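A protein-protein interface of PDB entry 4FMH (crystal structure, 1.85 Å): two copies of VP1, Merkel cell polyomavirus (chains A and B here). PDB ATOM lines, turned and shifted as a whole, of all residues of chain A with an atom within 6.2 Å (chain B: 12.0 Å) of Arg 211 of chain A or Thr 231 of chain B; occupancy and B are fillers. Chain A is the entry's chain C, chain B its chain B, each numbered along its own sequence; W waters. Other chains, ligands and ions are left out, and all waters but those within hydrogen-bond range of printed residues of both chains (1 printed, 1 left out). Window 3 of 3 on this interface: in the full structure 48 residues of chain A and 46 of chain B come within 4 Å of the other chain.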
ATOM      1  N   PHE A 135      20.268   1.535  12.001  1.00  0.00           N
ATOM      2  CA  PHE A 135      21.042   0.571  12.753  1.00  0.00           C
ATOM      3  C   PHE A 135      20.256  -0.727  12.852  1.00  0.00           C
ATOM      4  O   PHE A 135      19.022  -0.742  12.696  1.00  0.00           O
ATOM      5  CB  PHE A 135      21.462   1.112  14.135  1.00  0.00           C
ATOM      6  CG  PHE A 135      20.336   1.225  15.126  1.00  0.00           C
ATOM      7  CD1 PHE A 135      19.561   2.381  15.196  1.00  0.00           C
ATOM      8  CD2 PHE A 135      20.056   0.177  16.007  1.00  0.00           C
ATOM      9  CE1 PHE A 135      18.513   2.484  16.122  1.00  0.00           C
ATOM     10  CE2 PHE A 135      19.018   0.278  16.938  1.00  0.00           C
ATOM     11  CZ  PHE A 135      18.244   1.425  16.990  1.00  0.00           C
ATOM     12  N   ALA A 136      20.978  -1.812  13.092  1.00  0.00           N
ATOM     13  CA  ALA A 136      20.357  -3.120  13.243  1.00  0.00           C
ATOM     14  C   ALA A 136      21.108  -3.943  14.256  1.00  0.00           C
ATOM     15  O   ALA A 136      22.338  -3.847  14.373  1.00  0.00           O
ATOM     16  CB  ALA A 136      20.298  -3.846  11.902  1.00  0.00           C
ATOM     17  N   ILE A 137      20.353  -4.753  14.991  1.00  0.00           N
ATOM     18  CA  ILE A 137      20.917  -5.706  15.927  1.00  0.00           C
ATOM     19  C   ILE A 137      20.320  -7.058  15.550  1.00  0.00           C
ATOM     20  O   ILE A 137      19.107  -7.183  15.411  1.00  0.00           O
ATOM     21  CB  ILE A 137      20.562  -5.368  17.405  1.00  0.00           C
ATOM     22  CG1 ILE A 137      20.788  -3.875  17.728  1.00  0.00           C
ATOM     23  CG2 ILE A 137      21.357  -6.270  18.364  1.00  0.00           C
ATOM     24  CD1 ILE A 137      22.256  -3.382  17.611  1.00  0.00           C
ATOM     25  N   GLY A 138      21.170  -8.061  15.364  1.00  0.00           N
ATOM     26  CA  GLY A 138      20.679  -9.384  14.961  1.00  0.00           C
ATOM     27  C   GLY A 138      21.522 -10.531  15.457  1.00  0.00           C
ATOM     28  O   GLY A 138      22.670 -10.338  15.842  1.00  0.00           O
ATOM     29  N   LEU A 142      22.462  -9.211   8.635  1.00  0.00           N
ATOM     30  CA  LEU A 142      21.265  -8.546   8.124  1.00  0.00           C
ATOM     31  C   LEU A 142      21.015  -8.994   6.691  1.00  0.00           C
ATOM     32  O   LEU A 142      21.952  -9.069   5.879  1.00  0.00           O
ATOM     33  CB  LEU A 142      21.442  -7.024   8.171  1.00  0.00           C
ATOM     34  CG  LEU A 142      20.229  -6.131   7.871  1.00  0.00           C
ATOM     35  CD1 LEU A 142      19.189  -6.220   8.972  1.00  0.00           C
ATOM     36  CD2 LEU A 142      20.682  -4.686   7.688  1.00  0.00           C
ATOM     37  N   ASN A 207      14.968 -11.285   7.682  1.00  0.00           N
ATOM     38  CA  ASN A 207      15.319 -10.594   8.919  1.00  0.00           C
ATOM     39  C   ASN A 207      14.442 -10.907  10.136  1.00  0.00           C
ATOM     40  O   ASN A 207      14.271 -10.056  11.009  1.00  0.00           O
ATOM     41  CB  ASN A 207      15.387  -9.075   8.672  1.00  0.00           C
ATOM     42  CG  ASN A 207      16.653  -8.668   7.952  1.00  0.00           C
ATOM     43  OD1 ASN A 207      17.751  -9.026   8.374  1.00  0.00           O
ATOM     44  ND2 ASN A 207      16.510  -7.936   6.851  1.00  0.00           N
ATOM     45  N   GLU A 208      13.912 -12.129  10.209  1.00  0.00           N
ATOM     46  CA  GLU A 208      13.135 -12.556  11.383  1.00  0.00           C
ATOM     47  C   GLU A 208      13.962 -12.496  12.678  1.00  0.00           C
ATOM     48  O   GLU A 208      13.420 -12.271  13.764  1.00  0.00           O
ATOM     49  CB  GLU A 208      12.572 -13.969  11.196  1.00  0.00           C
ATOM     50  CG  GLU A 208      11.170 -14.014  10.565  1.00  0.00           C
ATOM     51  CD  GLU A 208      11.163 -14.511   9.121  1.00  0.00           C
ATOM     52  OE1 GLU A 208      10.376 -15.439   8.817  1.00  0.00           O
ATOM     53  OE2 GLU A 208      11.933 -13.982   8.289  1.00  0.00           O
ATOM     54  N   ASN A 209      15.270 -12.685  12.548  1.00  0.00           N
ATOM     55  CA  ASN A 209      16.170 -12.762  13.697  1.00  0.00           C
ATOM     56  C   ASN A 209      17.040 -11.498  13.873  1.00  0.00           C
ATOM     57  O   ASN A 209      18.109 -11.545  14.495  1.00  0.00           O
ATOM     58  CB  ASN A 209      17.032 -14.031  13.593  1.00  0.00           C
ATOM     59  CG  ASN A 209      17.677 -14.417  14.915  1.00  0.00           C
ATOM     60  OD1 ASN A 209      17.113 -14.188  15.986  1.00  0.00           O
ATOM     61  ND2 ASN A 209      18.871 -15.005  14.843  1.00  0.00           N
ATOM     62  N   SER A 210      16.569 -10.382  13.315  1.00  0.00           N
ATOM     63  CA  SER A 210      17.202  -9.068  13.488  1.00  0.00           C
ATOM     64  C   SER A 210      16.133  -8.014  13.749  1.00  0.00           C
ATOM     65  O   SER A 210      14.961  -8.230  13.431  1.00  0.00           O
ATOM     66  CB  SER A 210      17.980  -8.660  12.228  1.00  0.00           C
ATOM     67  OG  SER A 210      19.085  -9.506  11.988  1.00  0.00           O
ATOM     68  N   ARG A 211      16.544  -6.873  14.311  1.00  0.00           N
ATOM     69  CA  ARG A 211      15.679  -5.701  14.431  1.00  0.00           C
ATOM     70  C   ARG A 211      16.414  -4.553  13.756  1.00  0.00           C
ATOM     71  O   ARG A 211      17.592  -4.331  14.041  1.00  0.00           O
ATOM     72  CB  ARG A 211      15.433  -5.333  15.905  1.00  0.00           C
ATOM     73  CG  ARG A 211      14.981  -6.485  16.807  1.00  0.00           C
ATOM     74  CD  ARG A 211      13.587  -6.999  16.455  1.00  0.00           C
ATOM     75  NE  ARG A 211      13.248  -8.093  17.359  1.00  0.00           N
ATOM     76  CZ  ARG A 211      13.272  -9.384  17.052  1.00  0.00           C
ATOM     77  NH1 ARG A 211      13.597  -9.800  15.831  1.00  0.00           N
ATOM     78  NH2 ARG A 211      12.962 -10.268  17.988  1.00  0.00           N
ATOM     79  N   TYR A 212      15.740  -3.840  12.856  1.00  0.00           N
ATOM     80  CA  TYR A 212      16.370  -2.684  12.208  1.00  0.00           C
ATOM     81  C   TYR A 212      15.433  -1.490  12.175  1.00  0.00           C
ATOM     82  O   TYR A 212      14.217  -1.648  12.204  1.00  0.00           O
ATOM     83  CB  TYR A 212      16.893  -3.025  10.799  1.00  0.00           C
ATOM     84  CG  TYR A 212      15.831  -3.404   9.798  1.00  0.00           C
ATOM     85  CD1 TYR A 212      15.085  -2.418   9.132  1.00  0.00           C
ATOM     86  CD2 TYR A 212      15.574  -4.744   9.499  1.00  0.00           C
ATOM     87  CE1 TYR A 212      14.095  -2.762   8.211  1.00  0.00           C
ATOM     88  CE2 TYR A 212      14.595  -5.097   8.567  1.00  0.00           C
ATOM     89  CZ  TYR A 212      13.860  -4.101   7.933  1.00  0.00           C
ATOM     90  OH  TYR A 212      12.893  -4.433   7.015  1.00  0.00           O
ATOM     91  N   TYR A 213      16.030  -0.302  12.115  1.00  0.00           N
ATOM     92  CA  TYR A 213      15.340   0.970  12.252  1.00  0.00           C
ATOM     93  C   TYR A 213      16.125   1.950  11.406  1.00  0.00           C
ATOM     94  O   TYR A 213      17.335   2.094  11.577  1.00  0.00           O
ATOM     95  CB  TYR A 213      15.377   1.454  13.708  1.00  0.00           C
ATOM     96  CG  TYR A 213      15.083   0.382  14.730  1.00  0.00           C
ATOM     97  CD1 TYR A 213      13.814   0.264  15.285  1.00  0.00           C
ATOM     98  CD2 TYR A 213      16.077  -0.523  15.138  1.00  0.00           C
ATOM     99  CE1 TYR A 213      13.528  -0.725  16.217  1.00  0.00           C
ATOM    100  CE2 TYR A 213      15.799  -1.519  16.074  1.00  0.00           C
ATOM    101  CZ  TYR A 213      14.521  -1.606  16.608  1.00  0.00           C
ATOM    102  OH  TYR A 213      14.213  -2.576  17.535  1.00  0.00           O
ATOM    103  N   VAL A 235      14.021  -1.157  23.019  1.00  0.00           N
ATOM    104  CA  VAL A 235      13.681  -2.536  23.397  1.00  0.00           C
ATOM    105  C   VAL A 235      13.661  -3.391  22.122  1.00  0.00           C
ATOM    106  O   VAL A 235      13.045  -3.003  21.126  1.00  0.00           O
ATOM    107  CB  VAL A 235      12.309  -2.594  24.118  1.00  0.00           C
ATOM    108  CG1 VAL A 235      11.811  -4.031  24.279  1.00  0.00           C
ATOM    109  CG2 VAL A 235      12.382  -1.889  25.472  1.00  0.00           C
ATOM    110  N   LEU A 236      14.350  -4.535  22.162  1.00  0.00           N
ATOM    111  CA  LEU A 236      14.550  -5.395  20.986  1.00  0.00           C
ATOM    112  C   LEU A 236      13.617  -6.611  20.927  1.00  0.00           C
ATOM    113  O   LEU A 236      13.673  -7.404  19.976  1.00  0.00           O
ATOM    114  CB  LEU A 236      16.014  -5.848  20.897  1.00  0.00           C
ATOM    115  CG  LEU A 236      17.073  -4.756  20.689  1.00  0.00           C
ATOM    116  CD1 LEU A 236      18.484  -5.341  20.822  1.00  0.00           C
ATOM    117  CD2 LEU A 236      16.909  -4.056  19.337  1.00  0.00           C
ATOM    118  N   LEU A 237      12.758  -6.753  21.936  1.00  0.00           N
ATOM    119  CA  LEU A 237      11.820  -7.872  21.999  1.00  0.00           C
ATOM    120  C   LEU A 237      10.734  -7.728  20.929  1.00  0.00           C
ATOM    121  O   LEU A 237      10.267  -6.624  20.657  1.00  0.00           O
ATOM    122  CB  LEU A 237      11.184  -7.964  23.396  1.00  0.00           C
ATOM    123  CG  LEU A 237      12.126  -7.976  24.616  1.00  0.00           C
ATOM    124  CD1 LEU A 237      11.341  -8.078  25.937  1.00  0.00           C
ATOM    125  CD2 LEU A 237      13.173  -9.088  24.523  1.00  0.00           C
ATOM    126  N   ASP A 238      10.356  -8.839  20.309  1.00  0.00           N
ATOM    127  CA  ASP A 238       9.238  -8.833  19.373  1.00  0.00           C
ATOM    128  C   ASP A 238       7.908  -8.911  20.141  1.00  0.00           C
ATOM    129  O   ASP A 238       7.885  -8.774  21.368  1.00  0.00           O
ATOM    130  CB  ASP A 238       9.375  -9.962  18.337  1.00  0.00           C
ATOM    131  CG  ASP A 238       9.294 -11.364  18.952  1.00  0.00           C
ATOM    132  OD1 ASP A 238       8.928 -11.524  20.137  1.00  0.00           O
ATOM    133  OD2 ASP A 238       9.604 -12.323  18.224  1.00  0.00           O
ATOM    134  N   VAL A 242      10.430 -11.904  22.643  1.00  0.00           N
ATOM    135  CA  VAL A 242      11.674 -12.579  22.275  1.00  0.00           C
ATOM    136  C   VAL A 242      12.557 -11.639  21.444  1.00  0.00           C
ATOM    137  O   VAL A 242      12.112 -11.065  20.450  1.00  0.00           O
ATOM    138  CB  VAL A 242      11.409 -13.908  21.502  1.00  0.00           C
ATOM    139  CG1 VAL A 242      12.708 -14.630  21.199  1.00  0.00           C
ATOM    140  CG2 VAL A 242      10.470 -14.842  22.294  1.00  0.00           C
ATOM    141  N   GLY A 243      13.803 -11.470  21.875  1.00  0.00           N
ATOM    142  CA  GLY A 243      14.776 -10.700  21.119  1.00  0.00           C
ATOM    143  C   GLY A 243      15.536 -11.576  20.135  1.00  0.00           C
ATOM    144  O   GLY A 243      15.354 -12.793  20.129  1.00  0.00           O
ATOM    145  N   PRO A 244      16.389 -10.964  19.294  1.00  0.00           N
ATOM    146  CA  PRO A 244      17.254 -11.734  18.399  1.00  0.00           C
ATOM    147  C   PRO A 244      18.067 -12.767  19.181  1.00  0.00           C
ATOM    148  O   PRO A 244      18.591 -12.475  20.262  1.00  0.00           O
ATOM    149  CB  PRO A 244      18.180 -10.666  17.809  1.00  0.00           C
ATOM    150  CG  PRO A 244      17.320  -9.423  17.814  1.00  0.00           C
ATOM    151  CD  PRO A 244      16.591  -9.511  19.126  1.00  0.00           C
ATOM    152  N   SER B  96      -3.685  -7.790  11.379  1.00  0.00           N
ATOM    153  CA  SER B  96      -2.547  -6.873  11.426  1.00  0.00           C
ATOM    154  C   SER B  96      -1.709  -6.999  10.171  1.00  0.00           C
ATOM    155  O   SER B  96      -1.803  -7.992   9.446  1.00  0.00           O
ATOM    156  CB  SER B  96      -1.674  -7.130  12.663  1.00  0.00           C
ATOM    157  OG  SER B  96      -1.190  -8.463  12.685  1.00  0.00           O
ATOM    158  N   VAL B  97      -0.894  -5.976   9.922  1.00  0.00           N
ATOM    159  CA  VAL B  97      -0.001  -5.960   8.780  1.00  0.00           C
ATOM    160  C   VAL B  97       1.310  -5.277   9.148  1.00  0.00           C
ATOM    161  O   VAL B  97       1.319  -4.273   9.869  1.00  0.00           O
ATOM    162  CB  VAL B  97      -0.655  -5.275   7.534  1.00  0.00           C
ATOM    163  CG1 VAL B  97      -1.110  -3.847   7.852  1.00  0.00           C
ATOM    164  CG2 VAL B  97       0.288  -5.292   6.327  1.00  0.00           C
ATOM    165  N   LYS B  98       2.407  -5.849   8.669  1.00  0.00           N
ATOM    166  CA  LYS B  98       3.697  -5.177   8.658  1.00  0.00           C
ATOM    167  C   LYS B  98       3.949  -4.787   7.219  1.00  0.00           C
ATOM    168  O   LYS B  98       3.929  -5.635   6.323  1.00  0.00           O
ATOM    169  CB  LYS B  98       4.822  -6.098   9.137  1.00  0.00           C
ATOM    170  CG  LYS B  98       4.850  -6.343  10.627  1.00  0.00           C
ATOM    171  CD  LYS B  98       6.145  -7.027  11.017  1.00  0.00           C
ATOM    172  CE  LYS B  98       6.387  -6.949  12.509  1.00  0.00           C
ATOM    173  NZ  LYS B  98       7.666  -7.623  12.862  1.00  0.00           N
ATOM    174  N   THR B  99       4.187  -3.502   6.993  1.00  0.00           N
ATOM    175  CA  THR B  99       4.380  -3.012   5.638  1.00  0.00           C
ATOM    176  C   THR B  99       5.558  -2.048   5.599  1.00  0.00           C
ATOM    177  O   THR B  99       5.791  -1.304   6.550  1.00  0.00           O
ATOM    178  CB  THR B  99       3.068  -2.392   5.052  1.00  0.00           C
ATOM    179  OG1 THR B  99       3.268  -1.994   3.690  1.00  0.00           O
ATOM    180  CG2 THR B  99       2.585  -1.194   5.879  1.00  0.00           C
ATOM    181  N   GLU B 100       6.308  -2.088   4.501  1.00  0.00           N
ATOM    182  CA  GLU B 100       7.525  -1.306   4.367  1.00  0.00           C
ATOM    183  C   GLU B 100       7.713  -0.880   2.924  1.00  0.00           C
ATOM    184  O   GLU B 100       7.502  -1.683   2.003  1.00  0.00           O
ATOM    185  CB  GLU B 100       8.722  -2.154   4.820  1.00  0.00           C
ATOM    186  CG  GLU B 100      10.076  -1.441   4.797  1.00  0.00           C
ATOM    187  CD  GLU B 100      11.075  -2.092   5.736  1.00  0.00           C
ATOM    188  OE1 GLU B 100      10.757  -2.231   6.935  1.00  0.00           O
ATOM    189  OE2 GLU B 100      12.174  -2.472   5.282  1.00  0.00           O
ATOM    190  N   VAL B 101       8.078   0.387   2.724  1.00  0.00           N
ATOM    191  CA  VAL B 101       8.522   0.837   1.412  1.00  0.00           C
ATOM    192  C   VAL B 101       9.952   0.324   1.222  1.00  0.00           C
ATOM    193  O   VAL B 101      10.811   0.501   2.091  1.00  0.00           O
ATOM    194  CB  VAL B 101       8.420   2.383   1.255  1.00  0.00           C
ATOM    195  CG1 VAL B 101       8.881   2.825  -0.127  1.00  0.00           C
ATOM    196  CG2 VAL B 101       6.999   2.839   1.489  1.00  0.00           C
ATOM    197  N   GLN B 227      10.691   6.509   6.720  1.00  0.00           N
ATOM    198  CA  GLN B 227      11.245   5.586   7.707  1.00  0.00           C
ATOM    199  C   GLN B 227      11.007   4.144   7.285  1.00  0.00           C
ATOM    200  O   GLN B 227      10.116   3.855   6.486  1.00  0.00           O
ATOM    201  CB  GLN B 227      10.636   5.812   9.100  1.00  0.00           C
ATOM    202  CG  GLN B 227      10.920   7.191   9.713  1.00  0.00           C
ATOM    203  CD  GLN B 227       9.898   8.214   9.278  1.00  0.00           C
ATOM    204  OE1 GLN B 227       8.734   7.879   9.079  1.00  0.00           O
ATOM    205  NE2 GLN B 227      10.326   9.467   9.120  1.00  0.00           N
ATOM    206  N   PHE B 228      11.827   3.249   7.824  1.00  0.00           N
ATOM    207  CA  PHE B 228      11.672   1.815   7.622  1.00  0.00           C
ATOM    208  C   PHE B 228      12.149   1.082   8.869  1.00  0.00           C
ATOM    209  O   PHE B 228      13.137   1.474   9.483  1.00  0.00           O
ATOM    210  CB  PHE B 228      12.439   1.343   6.378  1.00  0.00           C
ATOM    211  CG  PHE B 228      13.884   1.811   6.318  1.00  0.00           C
ATOM    212  CD1 PHE B 228      14.199   3.105   5.876  1.00  0.00           C
ATOM    213  CD2 PHE B 228      14.920   0.954   6.663  1.00  0.00           C
ATOM    214  CE1 PHE B 228      15.526   3.543   5.813  1.00  0.00           C
ATOM    215  CE2 PHE B 228      16.253   1.382   6.605  1.00  0.00           C
ATOM    216  CZ  PHE B 228      16.553   2.684   6.173  1.00  0.00           C
ATOM    217  N   SER B 229      11.418   0.040   9.259  1.00  0.00           N
ATOM    218  CA  SER B 229      11.779  -0.787  10.404  1.00  0.00           C
ATOM    219  C   SER B 229      10.919  -2.030  10.357  1.00  0.00           C
ATOM    220  O   SER B 229       9.723  -1.949  10.057  1.00  0.00           O
ATOM    221  CB  SER B 229      11.504  -0.064  11.728  1.00  0.00           C
ATOM    222  OG  SER B 229      11.763  -0.920  12.838  1.00  0.00           O
ATOM    223  N   ASN B 230      11.505  -3.167  10.702  1.00  0.00           N
ATOM    224  CA  ASN B 230      10.729  -4.406  10.754  1.00  0.00           C
ATOM    225  C   ASN B 230      10.016  -4.628  12.096  1.00  0.00           C
ATOM    226  O   ASN B 230       9.552  -5.733  12.379  1.00  0.00           O
ATOM    227  CB  ASN B 230      11.593  -5.608  10.349  1.00  0.00           C
ATOM    228  CG  ASN B 230      12.716  -5.889  11.337  1.00  0.00           C
ATOM    229  OD1 ASN B 230      13.115  -5.011  12.109  1.00  0.00           O
ATOM    230  ND2 ASN B 230      13.224  -7.127  11.328  1.00  0.00           N
ATOM    231  N   THR B 231       9.927  -3.577  12.913  1.00  0.00           N
ATOM    232  CA  THR B 231       9.294  -3.675  14.228  1.00  0.00           C
ATOM    233  C   THR B 231       7.934  -2.982  14.287  1.00  0.00           C
ATOM    234  O   THR B 231       7.308  -2.946  15.347  1.00  0.00           O
ATOM    235  CB  THR B 231      10.181  -3.070  15.347  1.00  0.00           C
ATOM    236  OG1 THR B 231      10.313  -1.657  15.142  1.00  0.00           O
ATOM    237  CG2 THR B 231      11.563  -3.731  15.368  1.00  0.00           C
ATOM    238  N   LEU B 232       7.492  -2.422  13.165  1.00  0.00           N
ATOM    239  CA  LEU B 232       6.259  -1.630  13.144  1.00  0.00           C
ATOM    240  C   LEU B 232       5.079  -2.423  12.596  1.00  0.00           C
ATOM    241  O   LEU B 232       5.124  -2.919  11.469  1.00  0.00           O
ATOM    242  CB  LEU B 232       6.443  -0.354  12.314  1.00  0.00           C
ATOM    243  CG  LEU B 232       7.368   0.750  12.843  1.00  0.00           C
ATOM    244  CD1 LEU B 232       7.661   1.765  11.739  1.00  0.00           C
ATOM    245  CD2 LEU B 232       6.792   1.437  14.086  1.00  0.00           C
ATOM    246  N   THR B 233       4.019  -2.507  13.393  1.00  0.00           N
ATOM    247  CA  THR B 233       2.822  -3.262  13.036  1.00  0.00           C
ATOM    248  C   THR B 233       1.579  -2.368  13.067  1.00  0.00           C
ATOM    249  O   THR B 233       1.363  -1.641  14.035  1.00  0.00           O
ATOM    250  CB  THR B 233       2.616  -4.446  14.003  1.00  0.00           C
ATOM    251  OG1 THR B 233       3.772  -5.292  13.987  1.00  0.00           O
ATOM    252  CG2 THR B 233       1.389  -5.263  13.614  1.00  0.00           C
ATOM    253  N   THR B 234       0.771  -2.429  12.006  1.00  0.00           N
ATOM    254  CA  THR B 234      -0.535  -1.776  11.989  1.00  0.00           C
ATOM    255  C   THR B 234      -1.624  -2.794  12.337  1.00  0.00           C
ATOM    256  O   THR B 234      -1.718  -3.849  11.710  1.00  0.00           O
ATOM    257  CB  THR B 234      -0.840  -1.148  10.611  1.00  0.00           C
ATOM    258  OG1 THR B 234       0.176  -0.192  10.280  1.00  0.00           O
ATOM    259  CG2 THR B 234      -2.191  -0.458  10.615  1.00  0.00           C
ATOM    260  N   VAL B 235      -2.432  -2.469  13.338  1.00  0.00           N
ATOM    261  CA  VAL B 235      -3.548  -3.313  13.746  1.00  0.00           C
ATOM    262  C   VAL B 235      -4.757  -2.933  12.892  1.00  0.00           C
ATOM    263  O   VAL B 235      -5.050  -1.745  12.721  1.00  0.00           O
ATOM    264  CB  VAL B 235      -3.848  -3.152  15.261  1.00  0.00           C
ATOM    265  CG1 VAL B 235      -5.112  -3.902  15.659  1.00  0.00           C
ATOM    266  CG2 VAL B 235      -2.659  -3.645  16.095  1.00  0.00           C
ATOM    267  N   TYR B 277       6.375  -3.709   0.443  1.00  0.00           N
ATOM    268  CA  TYR B 277       6.242  -5.054   0.973  1.00  0.00           C
ATOM    269  C   TYR B 277       5.140  -5.123   2.026  1.00  0.00           C
ATOM    270  O   TYR B 277       4.934  -4.165   2.772  1.00  0.00           O
ATOM    271  CB  TYR B 277       7.585  -5.505   1.570  1.00  0.00           C
ATOM    272  CG  TYR B 277       7.480  -6.753   2.410  1.00  0.00           C
ATOM    273  CD1 TYR B 277       7.496  -8.017   1.821  1.00  0.00           C
ATOM    274  CD2 TYR B 277       7.339  -6.669   3.796  1.00  0.00           C
ATOM    275  CE1 TYR B 277       7.384  -9.171   2.595  1.00  0.00           C
ATOM    276  CE2 TYR B 277       7.230  -7.818   4.576  1.00  0.00           C
ATOM    277  CZ  TYR B 277       7.257  -9.057   3.968  1.00  0.00           C
ATOM    278  OH  TYR B 277       7.149 -10.186   4.747  1.00  0.00           O
ATOM    279  N   ASN B 279       3.360  -7.987   4.971  1.00  0.00           N
ATOM    280  CA  ASN B 279       3.148  -9.252   5.682  1.00  0.00           C
ATOM    281  C   ASN B 279       1.864  -9.131   6.516  1.00  0.00           C
ATOM    282  O   ASN B 279       1.850  -8.462   7.548  1.00  0.00           O
ATOM    283  CB  ASN B 279       4.354  -9.596   6.570  1.00  0.00           C
ATOM    284  CG  ASN B 279       4.299 -11.021   7.128  1.00  0.00           C
ATOM    285  OD1 ASN B 279       3.252 -11.500   7.553  1.00  0.00           O
ATOM    286  ND2 ASN B 279       5.438 -11.694   7.132  1.00  0.00           N
ATOM    287  N   THR B 281      -1.225 -10.708   8.765  1.00  0.00           N
ATOM    288  CA  THR B 281      -1.638 -11.802   9.640  1.00  0.00           C
ATOM    289  C   THR B 281      -3.150 -11.920   9.598  1.00  0.00           C
ATOM    290  O   THR B 281      -3.861 -10.929   9.778  1.00  0.00           O
ATOM    291  CB  THR B 281      -1.174 -11.573  11.102  1.00  0.00           C
ATOM    292  OG1 THR B 281       0.252 -11.490  11.138  1.00  0.00           O
ATOM    293  CG2 THR B 281      -1.625 -12.710  12.019  1.00  0.00           C
HETATM  294  O   HOH W   1      11.766  -8.635   9.145  1.00  0.00           O
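The side-chain amide nitrogen (ND2) of Asn 230 of chain B sits at hydrogen-bond distance from the backbone carbonyl oxygen (O) of Ser 210 of chain A (2.9 Å).
The backbone carbonyl oxygen (O) of Tyr 212 of chain A is in hydrogen-bond range of the side-chain hydroxyl (OG) of Ser 229 of chain B.
The backbone NH of Tyr 212 of chain A lies within hydrogen-bond range of the side-chain amide oxygen of Asn 230 of chain B (3.0 Å).
O of Asn 207 of chain A is in hydrogen-bond range of ND2 of Asn 230 of chain B (3.1 Å).
The side-chain carboxylate (OE2) of Glu 100 of chain B lies within hydrogen-bond range of the side-chain hydroxyl (OH) of Tyr 212 of chain A (2.7 Å).
The side-chain hydroxyl (OG1) of Thr 231 of chain B sits at hydrogen-bond distance from the side-chain hydroxyl (OG) of Ser 229 of chain B.
O of Glu 100 of chain B is in hydrogen-bond range of N of Tyr 277 of chain B (2.8 Å).
The backbone carbonyl oxygen (O) of Ile 137 of chain A sits at hydrogen-bond distance from the backbone NH (N) of Arg 211 of chain A.
N of Phe 135 of chain A is in hydrogen-bond range of O of Tyr 213 of chain A (3.0 Å).
The backbone carbonyl oxygen (O) of Asn 230 of chain B is in hydrogen-bond range of the side-chain amino group (NZ) of Lys 98 of chain B (2.7 Å).
OE1 of Glu 100 of chain B sits at hydrogen-bond distance from N of Ser 229 of chain B, at 3.3 Å.
CA of Arg 211 of chain A touches OD1 of Asn 230 of chain B, 3.5 Å away.
CD of Arg 211 of chain A touches CG2 of Thr 231 of chain B, at 3.99 Å.
Phe 228 of chain B touches Tyr 213 of chain A (O to CA, 3.6 Å).
CD1 of Tyr 213 of chain A touches OG of Ser 229 of chain B, 3.4 Å away.
CE1 of Tyr 213 of chain A touches OG1 of Thr 231 of chain B, at 3.5 Å.
No residue of chain B comes within 4 Å of Phe 135 of chain A.
Ala 136 of chain A touches none of the printed residues of chain B.
No residue of chain B comes within 4 Å of Ile 137 of chain A.
No residue of chain B comes within 4 Å of Gly 138 of chain A.
Printed residues of chain B within 4 Å of Asn 207 of chain A: Asn 230.
No residue of chain B comes within 4 Å of Asn 209 of chain A.
Printed residues of chain B within 4 Å of Arg 211 of chain A: Asn 230 (3.5 Å) and Thr 231 (3.99 Å).
Of chain B, only Glu 100 (2.7 Å), Ser 229 (2.6 Å) and Asn 230 (3.0 Å) come within 4 Å of Tyr 212 of chain A.
No residue of chain B comes within 4 Å of Val 242 of chain A.
No residue of chain B comes within 4 Å of Gly 243 of chain A.
No residue of chain B comes within 4 Å of Pro 244 of chain A.
Printed residues of chain A within 4 Å of Glu 100 of chain B: Tyr 212 (2.7 Å).
Printed residues of chain A within 4 Å of Phe 228 of chain B: Tyr 213 (3.6 Å).
Printed residues of chain A within 4 Å of Ser 229 of chain B: Tyr 212 (2.6 Å) and Tyr 213 (3.4 Å).
Printed residues of chain A within 4 Å of Asn 230 of chain B: Asn 207, Ser 210, Arg 211 and Tyr 212.
Of the printed residues of chain A, Thr 231 of chain B touches Arg 211 (3.99 Å) and Tyr 213 (3.5 Å).
Thr 233 of chain B touches none of the printed residues of chain A.
The nearest printed residue of chain A that does not touch Thr 231 of chain B is Tyr 212 of chain A (4.6 Å).
Printed residues of chain B that touch a printed residue of chain A: Glu 100, Phe 228, Ser 229, Asn 230 and Thr 231.
Along chain B the printed residues that touch a printed residue of chain A span positions 100 to 231.
Of the 19 printed residues of chain A, 5 touch a printed residue of chain B.
Hydrophobic or aromatic side chains of chain A within 4 Å of the printed part of chain B: Tyr 212 and Tyr 213.
Among the printed residues, no Asp or Glu carboxylate lies within 4 Å of a Lys or Arg side-chain nitrogen of the other chain.
Position printed for both chains: 235.
Water W1 bridges ND2 of Asn 230 of chain B (3.0 Å) and O of Asn 207 of chain A (3.4 Å).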
